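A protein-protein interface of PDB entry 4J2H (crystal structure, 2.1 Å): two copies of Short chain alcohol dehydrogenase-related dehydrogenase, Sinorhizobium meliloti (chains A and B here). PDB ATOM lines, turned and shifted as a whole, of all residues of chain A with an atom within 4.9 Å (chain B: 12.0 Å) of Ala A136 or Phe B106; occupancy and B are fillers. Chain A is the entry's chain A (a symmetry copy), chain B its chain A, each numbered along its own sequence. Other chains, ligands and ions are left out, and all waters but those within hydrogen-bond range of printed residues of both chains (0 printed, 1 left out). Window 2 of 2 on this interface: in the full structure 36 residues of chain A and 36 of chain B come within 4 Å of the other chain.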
ATOM      1  N   GLN A 129      28.790 -16.250 -22.814  1.00  0.00           N
ATOM      2  CA  GLN A 129      28.476 -15.219 -23.768  1.00  0.00           C
ATOM      3  C   GLN A 129      29.750 -14.548 -24.306  1.00  0.00           C
ATOM      4  O   GLN A 129      29.955 -14.483 -25.517  1.00  0.00           O
ATOM      5  CB  GLN A 129      27.534 -14.199 -23.128  1.00  0.00           C
ATOM      6  CG  GLN A 129      27.284 -12.953 -23.969  1.00  0.00           C
ATOM      7  CD  GLN A 129      26.539 -11.898 -23.211  1.00  0.00           C
ATOM      8  OE1 GLN A 129      27.133 -11.152 -22.430  1.00  0.00           O
ATOM      9  NE2 GLN A 129      25.235 -11.796 -23.454  1.00  0.00           N
ATOM     10  N   GLY A 132      31.986 -17.242 -26.077  1.00  0.00           N
ATOM     11  CA  GLY A 132      31.189 -17.485 -27.274  1.00  0.00           C
ATOM     12  C   GLY A 132      31.378 -16.468 -28.393  1.00  0.00           C
ATOM     13  O   GLY A 132      31.590 -16.855 -29.540  1.00  0.00           O
ATOM     14  N   ARG A 133      31.297 -15.176 -28.062  1.00  0.00           N
ATOM     15  CA  ARG A 133      31.394 -14.105 -29.076  1.00  0.00           C
ATOM     16  C   ARG A 133      32.767 -14.107 -29.738  1.00  0.00           C
ATOM     17  O   ARG A 133      32.873 -13.903 -30.952  1.00  0.00           O
ATOM     18  CB  ARG A 133      31.096 -12.723 -28.474  1.00  0.00           C
ATOM     19  CG  ARG A 133      30.937 -11.617 -29.518  1.00  0.00           C
ATOM     20  CD  ARG A 133      30.720 -10.237 -28.902  1.00  0.00           C
ATOM     21  NE  ARG A 133      29.409 -10.112 -28.253  1.00  0.00           N
ATOM     22  CZ  ARG A 133      29.157 -10.318 -26.955  1.00  0.00           C
ATOM     23  NH1 ARG A 133      27.915 -10.182 -26.494  1.00  0.00           N
ATOM     24  NH2 ARG A 133      30.124 -10.662 -26.105  1.00  0.00           N
ATOM     25  N   ILE A 134      33.806 -14.338 -28.935  1.00  0.00           N
ATOM     26  CA  ILE A 134      35.172 -14.481 -29.434  1.00  0.00           C
ATOM     27  C   ILE A 134      35.276 -15.694 -30.346  1.00  0.00           C
ATOM     28  O   ILE A 134      35.869 -15.621 -31.414  1.00  0.00           O
ATOM     29  CB  ILE A 134      36.202 -14.629 -28.293  1.00  0.00           C
ATOM     30  CG1 ILE A 134      36.308 -13.323 -27.501  1.00  0.00           C
ATOM     31  CG2 ILE A 134      37.573 -15.006 -28.851  1.00  0.00           C
ATOM     32  CD1 ILE A 134      37.167 -13.414 -26.257  1.00  0.00           C
ATOM     33  N   MET A 135      34.706 -16.811 -29.920  1.00  0.00           N
ATOM     34  CA  MET A 135      34.748 -18.038 -30.722  1.00  0.00           C
ATOM     35  C   MET A 135      33.983 -17.859 -32.018  1.00  0.00           C
ATOM     36  O   MET A 135      34.382 -18.376 -33.062  1.00  0.00           O
ATOM     37  CB  MET A 135      34.129 -19.205 -29.952  1.00  0.00           C
ATOM     38  CG  MET A 135      35.026 -19.705 -28.814  1.00  0.00           C
ATOM     39  SD  MET A 135      34.034 -21.073 -27.803  1.00  0.00           S
ATOM     40  CE  MET A 135      35.244 -21.143 -26.244  1.00  0.00           C
ATOM     41  N   ALA A 136      32.863 -17.142 -31.945  1.00  0.00           N
ATOM     42  CA  ALA A 136      31.984 -16.973 -33.087  1.00  0.00           C
ATOM     43  C   ALA A 136      32.655 -16.081 -34.130  1.00  0.00           C
ATOM     44  O   ALA A 136      32.477 -16.298 -35.308  1.00  0.00           O
ATOM     45  CB  ALA A 136      30.635 -16.394 -32.663  1.00  0.00           C
ATOM     46  N   ASP A 137      33.437 -15.102 -33.685  1.00  0.00           N
ATOM     47  CA  ASP A 137      34.170 -14.236 -34.598  1.00  0.00           C
ATOM     48  C   ASP A 137      35.366 -14.939 -35.228  1.00  0.00           C
ATOM     49  O   ASP A 137      35.792 -14.534 -36.296  1.00  0.00           O
ATOM     50  CB  ASP A 137      34.622 -12.947 -33.905  1.00  0.00           C
ATOM     51  CG  ASP A 137      33.456 -12.100 -33.429  1.00  0.00           C
ATOM     52  OD1 ASP A 137      32.330 -12.282 -33.928  1.00  0.00           O
ATOM     53  OD2 ASP A 137      33.659 -11.257 -32.535  1.00  0.00           O
ATOM     54  N   ALA A 138      35.903 -15.979 -34.588  1.00  0.00           N
ATOM     55  CA  ALA A 138      36.987 -16.783 -35.191  1.00  0.00           C
ATOM     56  C   ALA A 138      36.390 -18.075 -35.769  1.00  0.00           C
ATOM     57  O   ALA A 138      35.478 -17.983 -36.576  1.00  0.00           O
ATOM     58  CB  ALA A 138      38.107 -17.048 -34.190  1.00  0.00           C
ATOM     59  N   GLY A 140      35.068 -20.946 -33.992  1.00  0.00           N
ATOM     60  CA  GLY A 140      34.303 -21.765 -33.064  1.00  0.00           C
ATOM     61  C   GLY A 140      35.110 -22.335 -31.908  1.00  0.00           C
ATOM     62  O   GLY A 140      36.181 -21.869 -31.603  1.00  0.00           O
ATOM     63  N   GLU A 178      21.559 -23.142 -30.068  1.00  0.00           N
ATOM     64  CA  GLU A 178      21.718 -21.832 -30.660  1.00  0.00           C
ATOM     65  C   GLU A 178      23.079 -21.637 -31.304  1.00  0.00           C
ATOM     66  O   GLU A 178      23.181 -20.956 -32.303  1.00  0.00           O
ATOM     67  CB  GLU A 178      21.500 -20.742 -29.608  1.00  0.00           C
ATOM     68  CG  GLU A 178      21.500 -19.308 -30.179  1.00  0.00           C
ATOM     69  CD  GLU A 178      21.159 -18.279 -29.120  1.00  0.00           C
ATOM     70  OE1 GLU A 178      20.810 -18.699 -27.977  1.00  0.00           O
ATOM     71  OE2 GLU A 178      21.225 -17.058 -29.421  1.00  0.00           O
ATOM     72  N   TRP A 179      24.141 -22.213 -30.749  1.00  0.00           N
ATOM     73  CA  TRP A 179      25.478 -21.863 -31.227  1.00  0.00           C
ATOM     74  C   TRP A 179      26.179 -22.919 -32.084  1.00  0.00           C
ATOM     75  O   TRP A 179      27.315 -22.705 -32.532  1.00  0.00           O
ATOM     76  CB  TRP A 179      26.387 -21.432 -30.083  1.00  0.00           C
ATOM     77  CG  TRP A 179      26.069 -20.127 -29.462  1.00  0.00           C
ATOM     78  CD1 TRP A 179      25.271 -19.135 -29.962  1.00  0.00           C
ATOM     79  CD2 TRP A 179      26.590 -19.632 -28.225  1.00  0.00           C
ATOM     80  NE1 TRP A 179      25.240 -18.067 -29.099  1.00  0.00           N
ATOM     81  CE2 TRP A 179      26.055 -18.336 -28.034  1.00  0.00           C
ATOM     82  CE3 TRP A 179      27.458 -20.159 -27.258  1.00  0.00           C
ATOM     83  CZ2 TRP A 179      26.357 -17.562 -26.910  1.00  0.00           C
ATOM     84  CZ3 TRP A 179      27.759 -19.398 -26.152  1.00  0.00           C
ATOM     85  CH2 TRP A 179      27.214 -18.102 -25.986  1.00  0.00           C
ATOM     86  N   HIS A 182      27.648 -21.635 -35.207  1.00  0.00           N
ATOM     87  CA  HIS A 182      28.921 -20.921 -35.121  1.00  0.00           C
ATOM     88  C   HIS A 182      30.101 -21.873 -34.881  1.00  0.00           C
ATOM     89  O   HIS A 182      31.212 -21.441 -34.573  1.00  0.00           O
ATOM     90  CB  HIS A 182      28.857 -19.894 -34.002  1.00  0.00           C
ATOM     91  CG  HIS A 182      27.840 -18.822 -34.226  1.00  0.00           C
ATOM     92  ND1 HIS A 182      28.004 -17.831 -35.162  1.00  0.00           N
ATOM     93  CD2 HIS A 182      26.657 -18.573 -33.622  1.00  0.00           C
ATOM     94  CE1 HIS A 182      26.962 -17.019 -35.133  1.00  0.00           C
ATOM     95  NE2 HIS A 182      26.134 -17.446 -34.204  1.00  0.00           N
ATOM     96  N   ILE A 184      30.389 -23.862 -32.350  1.00  0.00           N
ATOM     97  CA  ILE A 184      30.628 -23.884 -30.917  1.00  0.00           C
ATOM     98  C   ILE A 184      29.807 -25.033 -30.333  1.00  0.00           C
ATOM     99  O   ILE A 184      28.591 -25.002 -30.397  1.00  0.00           O
ATOM    100  CB  ILE A 184      30.212 -22.567 -30.223  1.00  0.00           C
ATOM    101  CG1 ILE A 184      30.974 -21.379 -30.781  1.00  0.00           C
ATOM    102  CG2 ILE A 184      30.462 -22.658 -28.708  1.00  0.00           C
ATOM    103  CD1 ILE A 184      30.396 -20.046 -30.362  1.00  0.00           C
ATOM    104  N   ASN B 101      10.523 -14.773 -22.945  1.00  0.00           N
ATOM    105  CA  ASN B 101      11.376 -13.905 -23.768  1.00  0.00           C
ATOM    106  C   ASN B 101      12.260 -14.689 -24.723  1.00  0.00           C
ATOM    107  O   ASN B 101      12.737 -15.777 -24.393  1.00  0.00           O
ATOM    108  CB  ASN B 101      12.237 -12.998 -22.874  1.00  0.00           C
ATOM    109  CG  ASN B 101      13.153 -12.083 -23.664  1.00  0.00           C
ATOM    110  OD1 ASN B 101      14.213 -12.488 -24.141  1.00  0.00           O
ATOM    111  ND2 ASN B 101      12.763 -10.836 -23.779  1.00  0.00           N
ATOM    112  N   VAL B 102      12.450 -14.132 -25.913  1.00  0.00           N
ATOM    113  CA  VAL B 102      13.460 -14.594 -26.846  1.00  0.00           C
ATOM    114  C   VAL B 102      14.386 -13.430 -27.189  1.00  0.00           C
ATOM    115  O   VAL B 102      13.934 -12.309 -27.362  1.00  0.00           O
ATOM    116  CB  VAL B 102      12.843 -15.226 -28.110  1.00  0.00           C
ATOM    117  CG1 VAL B 102      12.157 -16.535 -27.750  1.00  0.00           C
ATOM    118  CG2 VAL B 102      11.881 -14.273 -28.817  1.00  0.00           C
ATOM    119  N   ARG B 103      15.680 -13.708 -27.262  1.00  0.00           N
ATOM    120  CA  ARG B 103      16.699 -12.702 -27.507  1.00  0.00           C
ATOM    121  C   ARG B 103      17.987 -13.445 -27.824  1.00  0.00           C
ATOM    122  O   ARG B 103      18.406 -14.315 -27.053  1.00  0.00           O
ATOM    123  CB  ARG B 103      16.920 -11.818 -26.270  1.00  0.00           C
ATOM    124  CG  ARG B 103      17.909 -10.653 -26.475  1.00  0.00           C
ATOM    125  CD  ARG B 103      17.321  -9.518 -27.297  1.00  0.00           C
ATOM    126  NE  ARG B 103      15.944  -9.281 -26.855  1.00  0.00           N
ATOM    127  CZ  ARG B 103      15.529  -8.312 -26.036  1.00  0.00           C
ATOM    128  NH1 ARG B 103      16.364  -7.381 -25.574  1.00  0.00           N
ATOM    129  NH2 ARG B 103      14.238  -8.269 -25.697  1.00  0.00           N
ATOM    130  N   PRO B 104      18.609 -13.150 -28.972  1.00  0.00           N
ATOM    131  CA  PRO B 104      19.900 -13.784 -29.210  1.00  0.00           C
ATOM    132  C   PRO B 104      20.822 -13.693 -27.976  1.00  0.00           C
ATOM    133  O   PRO B 104      20.999 -12.620 -27.410  1.00  0.00           O
ATOM    134  CB  PRO B 104      20.461 -12.993 -30.389  1.00  0.00           C
ATOM    135  CG  PRO B 104      19.248 -12.512 -31.123  1.00  0.00           C
ATOM    136  CD  PRO B 104      18.220 -12.237 -30.072  1.00  0.00           C
ATOM    137  N   SER B 105      21.393 -14.821 -27.572  1.00  0.00           N
ATOM    138  CA  SER B 105      22.206 -14.901 -26.347  1.00  0.00           C
ATOM    139  C   SER B 105      23.424 -13.968 -26.316  1.00  0.00           C
ATOM    140  O   SER B 105      23.838 -13.539 -25.236  1.00  0.00           O
ATOM    141  CB  SER B 105      22.643 -16.345 -26.094  1.00  0.00           C
ATOM    142  OG  SER B 105      21.529 -17.182 -25.847  1.00  0.00           O
ATOM    143  N   PHE B 106      23.991 -13.644 -27.483  1.00  0.00           N
ATOM    144  CA  PHE B 106      25.051 -12.625 -27.561  1.00  0.00           C
ATOM    145  C   PHE B 106      24.546 -11.232 -27.202  1.00  0.00           C
ATOM    146  O   PHE B 106      25.344 -10.355 -26.886  1.00  0.00           O
ATOM    147  CB  PHE B 106      25.693 -12.568 -28.957  1.00  0.00           C
ATOM    148  CG  PHE B 106      26.470 -13.800 -29.332  1.00  0.00           C
ATOM    149  CD1 PHE B 106      27.337 -14.402 -28.432  1.00  0.00           C
ATOM    150  CD2 PHE B 106      26.359 -14.340 -30.605  1.00  0.00           C
ATOM    151  CE1 PHE B 106      28.060 -15.531 -28.784  1.00  0.00           C
ATOM    152  CE2 PHE B 106      27.072 -15.473 -30.962  1.00  0.00           C
ATOM    153  CZ  PHE B 106      27.927 -16.070 -30.053  1.00  0.00           C
ATOM    154  N   ASP B 107      23.223 -11.043 -27.254  1.00  0.00           N
ATOM    155  CA  ASP B 107      22.575  -9.745 -27.017  1.00  0.00           C
ATOM    156  C   ASP B 107      21.821  -9.663 -25.692  1.00  0.00           C
ATOM    157  O   ASP B 107      21.150  -8.670 -25.446  1.00  0.00           O
ATOM    158  CB  ASP B 107      21.561  -9.460 -28.126  1.00  0.00           C
ATOM    159  CG  ASP B 107      22.194  -9.336 -29.489  1.00  0.00           C
ATOM    160  OD1 ASP B 107      23.419  -9.127 -29.584  1.00  0.00           O
ATOM    161  OD2 ASP B 107      21.444  -9.438 -30.475  1.00  0.00           O
ATOM    162  N   VAL B 108      21.905 -10.701 -24.854  1.00  0.00           N
ATOM    163  CA  VAL B 108      21.284 -10.672 -23.516  1.00  0.00           C
ATOM    164  C   VAL B 108      22.165  -9.830 -22.602  1.00  0.00           C
ATOM    165  O   VAL B 108      23.359 -10.098 -22.479  1.00  0.00           O
ATOM    166  CB  VAL B 108      21.134 -12.096 -22.927  1.00  0.00           C
ATOM    167  CG1 VAL B 108      20.626 -12.060 -21.490  1.00  0.00           C
ATOM    168  CG2 VAL B 108      20.181 -12.917 -23.780  1.00  0.00           C
ATOM    169  N   ASP B 109      21.597  -8.796 -21.995  1.00  0.00           N
ATOM    170  CA  ASP B 109      22.333  -7.992 -21.017  1.00  0.00           C
ATOM    171  C   ASP B 109      21.916  -8.393 -19.598  1.00  0.00           C
ATOM    172  O   ASP B 109      21.011  -9.225 -19.417  1.00  0.00           O
ATOM    173  CB  ASP B 109      22.167  -6.476 -21.272  1.00  0.00           C
ATOM    174  CG  ASP B 109      20.753  -5.968 -21.038  1.00  0.00           C
ATOM    175  OD1 ASP B 109      19.821  -6.771 -20.866  1.00  0.00           O
ATOM    176  OD2 ASP B 109      20.570  -4.733 -21.041  1.00  0.00           O
ATOM    177  N   GLU B 110      22.594  -7.818 -18.605  1.00  0.00           N
ATOM    178  CA  GLU B 110      22.376  -8.188 -17.208  1.00  0.00           C
ATOM    179  C   GLU B 110      20.910  -8.049 -16.791  1.00  0.00           C
ATOM    180  O   GLU B 110      20.344  -8.937 -16.135  1.00  0.00           O
ATOM    181  CB  GLU B 110      23.246  -7.332 -16.277  1.00  0.00           C
ATOM    182  CG  GLU B 110      22.970  -7.642 -14.807  1.00  0.00           C
ATOM    183  CD  GLU B 110      24.047  -7.141 -13.870  1.00  0.00           C
ATOM    184  OE1 GLU B 110      24.595  -6.053 -14.120  1.00  0.00           O
ATOM    185  OE2 GLU B 110      24.325  -7.834 -12.870  1.00  0.00           O
ATOM    186  N   ALA B 111      20.327  -6.924 -17.189  1.00  0.00           N
ATOM    187  CA  ALA B 111      19.001  -6.520 -16.779  1.00  0.00           C
ATOM    188  C   ALA B 111      17.955  -7.481 -17.281  1.00  0.00           C
ATOM    189  O   ALA B 111      17.029  -7.839 -16.557  1.00  0.00           O
ATOM    190  CB  ALA B 111      18.713  -5.114 -17.292  1.00  0.00           C
ATOM    191  N   LEU B 112      18.099  -7.903 -18.529  1.00  0.00           N
ATOM    192  CA  LEU B 112      17.172  -8.854 -19.100  1.00  0.00           C
ATOM    193  C   LEU B 112      17.258 -10.184 -18.342  1.00  0.00           C
ATOM    194  O   LEU B 112      16.230 -10.742 -17.927  1.00  0.00           O
ATOM    195  CB  LEU B 112      17.465  -9.043 -20.587  1.00  0.00           C
ATOM    196  CG  LEU B 112      16.542 -10.024 -21.309  1.00  0.00           C
ATOM    197  CD1 LEU B 112      15.088  -9.546 -21.255  1.00  0.00           C
ATOM    198  CD2 LEU B 112      17.043 -10.209 -22.738  1.00  0.00           C
ATOM    199  N   TRP B 113      18.485 -10.676 -18.154  1.00  0.00           N
ATOM    200  CA  TRP B 113      18.724 -11.897 -17.402  1.00  0.00           C
ATOM    201  C   TRP B 113      17.972 -11.849 -16.083  1.00  0.00           C
ATOM    202  O   TRP B 113      17.243 -12.772 -15.746  1.00  0.00           O
ATOM    203  CB  TRP B 113      20.220 -12.126 -17.129  1.00  0.00           C
ATOM    204  CG  TRP B 113      20.410 -13.274 -16.176  1.00  0.00           C
ATOM    205  CD1 TRP B 113      20.321 -13.225 -14.811  1.00  0.00           C
ATOM    206  CD2 TRP B 113      20.677 -14.638 -16.514  1.00  0.00           C
ATOM    207  NE1 TRP B 113      20.500 -14.479 -14.280  1.00  0.00           N
ATOM    208  CE2 TRP B 113      20.724 -15.368 -15.298  1.00  0.00           C
ATOM    209  CE3 TRP B 113      20.860 -15.321 -17.723  1.00  0.00           C
ATOM    210  CZ2 TRP B 113      20.962 -16.753 -15.256  1.00  0.00           C
ATOM    211  CZ3 TRP B 113      21.088 -16.698 -17.682  1.00  0.00           C
ATOM    212  CH2 TRP B 113      21.141 -17.401 -16.453  1.00  0.00           C
ATOM    213  N   ILE B 116      14.061 -11.956 -16.174  1.00  0.00           N
ATOM    214  CA  ILE B 116      13.585 -13.281 -16.513  1.00  0.00           C
ATOM    215  C   ILE B 116      13.762 -14.246 -15.333  1.00  0.00           C
ATOM    216  O   ILE B 116      12.831 -14.983 -14.993  1.00  0.00           O
ATOM    217  CB  ILE B 116      14.299 -13.848 -17.762  1.00  0.00           C
ATOM    218  CG1 ILE B 116      13.976 -12.994 -18.991  1.00  0.00           C
ATOM    219  CG2 ILE B 116      13.863 -15.286 -18.018  1.00  0.00           C
ATOM    220  CD1 ILE B 116      14.858 -13.281 -20.184  1.00  0.00           C
ATOM    221  N   ILE B 155      15.606 -24.213 -26.345  1.00  0.00           N
ATOM    222  CA  ILE B 155      15.140 -23.326 -27.422  1.00  0.00           C
ATOM    223  C   ILE B 155      16.171 -22.250 -27.669  1.00  0.00           C
ATOM    224  O   ILE B 155      16.450 -21.474 -26.764  1.00  0.00           O
ATOM    225  CB  ILE B 155      13.771 -22.690 -27.077  1.00  0.00           C
ATOM    226  CG1 ILE B 155      12.723 -23.794 -27.083  1.00  0.00           C
ATOM    227  CG2 ILE B 155      13.399 -21.564 -28.092  1.00  0.00           C
ATOM    228  CD1 ILE B 155      11.366 -23.420 -26.496  1.00  0.00           C
ATOM    229  N   PRO B 156      16.712 -22.167 -28.911  1.00  0.00           N
ATOM    230  CA  PRO B 156      17.669 -21.112 -29.226  1.00  0.00           C
ATOM    231  C   PRO B 156      17.060 -19.718 -29.000  1.00  0.00           C
ATOM    232  O   PRO B 156      15.869 -19.516 -29.220  1.00  0.00           O
ATOM    233  CB  PRO B 156      18.033 -21.365 -30.700  1.00  0.00           C
ATOM    234  CG  PRO B 156      16.910 -22.174 -31.260  1.00  0.00           C
ATOM    235  CD  PRO B 156      16.256 -22.895 -30.114  1.00  0.00           C
ATOM    236  N   THR B 157      17.877 -18.793 -28.510  1.00  0.00           N
ATOM    237  CA  THR B 157      17.437 -17.449 -28.078  1.00  0.00           C
ATOM    238  C   THR B 157      16.487 -17.391 -26.879  1.00  0.00           C
ATOM    239  O   THR B 157      16.038 -16.310 -26.505  1.00  0.00           O
ATOM    240  CB  THR B 157      16.836 -16.602 -29.239  1.00  0.00           C
ATOM    241  OG1 THR B 157      15.441 -16.892 -29.378  1.00  0.00           O
ATOM    242  CG2 THR B 157      17.573 -16.879 -30.548  1.00  0.00           C
ATOM    243  N   ALA B 158      16.184 -18.526 -26.262  1.00  0.00           N
ATOM    244  CA  ALA B 158      15.440 -18.538 -25.012  1.00  0.00           C
ATOM    245  C   ALA B 158      16.319 -19.124 -23.888  1.00  0.00           C
ATOM    246  O   ALA B 158      15.886 -19.997 -23.124  1.00  0.00           O
ATOM    247  CB  ALA B 158      14.150 -19.324 -25.172  1.00  0.00           C
ATOM    248  N   VAL B 159      17.536 -18.610 -23.772  1.00  0.00           N
ATOM    249  CA  VAL B 159      18.494 -19.203 -22.847  1.00  0.00           C
ATOM    250  C   VAL B 159      18.192 -18.868 -21.366  1.00  0.00           C
ATOM    251  O   VAL B 159      18.011 -19.782 -20.570  1.00  0.00           O
ATOM    252  CB  VAL B 159      19.950 -18.934 -23.281  1.00  0.00           C
ATOM    253  CG1 VAL B 159      20.934 -19.365 -22.198  1.00  0.00           C
ATOM    254  CG2 VAL B 159      20.252 -19.713 -24.568  1.00  0.00           C
ATOM    255  N   PRO B 160      18.105 -17.573 -21.003  1.00  0.00           N
ATOM    256  CA  PRO B 160      17.673 -17.214 -19.648  1.00  0.00           C
ATOM    257  C   PRO B 160      16.346 -17.854 -19.290  1.00  0.00           C
ATOM    258  O   PRO B 160      16.206 -18.410 -18.172  1.00  0.00           O
ATOM    259  CB  PRO B 160      17.547 -15.695 -19.697  1.00  0.00           C
ATOM    260  CG  PRO B 160      18.411 -15.271 -20.833  1.00  0.00           C
ATOM    261  CD  PRO B 160      18.365 -16.386 -21.832  1.00  0.00           C
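Gln A129 touches Phe B106 (NE2 to O, 3.7 Å). C of Gly A132 touches CE1 of Phe B106 (3.5 Å). CZ of Phe B106 touches CB of Ala A136, 3.8 Å away. Pro B104 touches Glu A178. Glu A178 touches Pro B156 (CB to CB, 3.7 Å). OE1 of Glu A178 touches CG2 of Val B159, 3.6 Å away. CB of Ser B105 touches CZ2 of Trp A179 (3.99 Å). CE1 of Phe B106 touches CZ2 of Trp A179, at 3.2 Å. NE2 of His A182 touches CE2 of Phe B106, 3.9 Å away.
Of the printed residues of chain B, Gln A129 touches Ser B105 (2.9 Å), Phe B106 (3.7 Å) and Val B108 (2.7 Å). Arg A133 touches one residue of chain B. Met A135 touches none of the printed residues of chain B. Ala A136 touches just one residue of chain B: Phe B106. No residue of chain B comes within 4 Å of Asp A137. No residue of chain B comes within 4 Å of Ala A138. No residue of chain B comes within 4 Å of Gly A140. Printed residues of chain B within 4 Å of Trp A179: Ser B105 and Phe B106. His A182 touches just one residue of chain B: Phe B106. Printed residues of chain A within 4 Å of Pro B104: Glu A178. Phe B106 touches six residues of chain A. Of the printed residues of chain A, Val B108 touches Gln A129 (2.7 Å). Printed residues of chain A within 4 Å of Pro B156: Glu A178 (3.7 Å). Of the printed residues of chain A, Val B159 touches Glu A178 (3.6 Å). The nearest residue of chain B that does not touch Ala A136 is Ser B105 (9.9 Å). The nearest printed residue of chain A that does not touch Thr B157 is Trp A179 (7.4 Å).
The side-chain amide nitrogen of Gln A129 sits at hydrogen-bond distance from the backbone carbonyl oxygen of Val B108. OE1 of Glu A178 sits at hydrogen-bond distance from N of Thr B157 (3.0 Å). The side-chain hydroxyl (OG) of Ser B105 lies within hydrogen-bond range of the side-chain carboxylate (OE1) of Glu A178, 2.7 Å away. O of Ser B105 lies within hydrogen-bond range of NE2 of Gln A129 (2.9 Å). O of Phe B106 lies within hydrogen-bond range of NH1 of Arg A133, 2.6 Å away.
No position is printed for both chains. Of the 14 pairs that touch across the chains among the printed residues, none has its exchanged pair printed and touching as well.
O of Trp A179 sits at hydrogen-bond distance from N of Ile A184, 3.3 Å away. N of Arg B103 lies within hydrogen-bond range of O of Thr B157 (2.7 Å).
Hydrophobic or aromatic side chains of chain B that line the printed part of chain A: Phe B106, Pro B156 and Val B159. Of the 13 printed residues of chain A, 7 touch a printed residue of chain B. Among the printed residues, no Asp or Glu carboxylate lies within 4 Å of a Lys or Arg side-chain nitrogen of the other chain.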
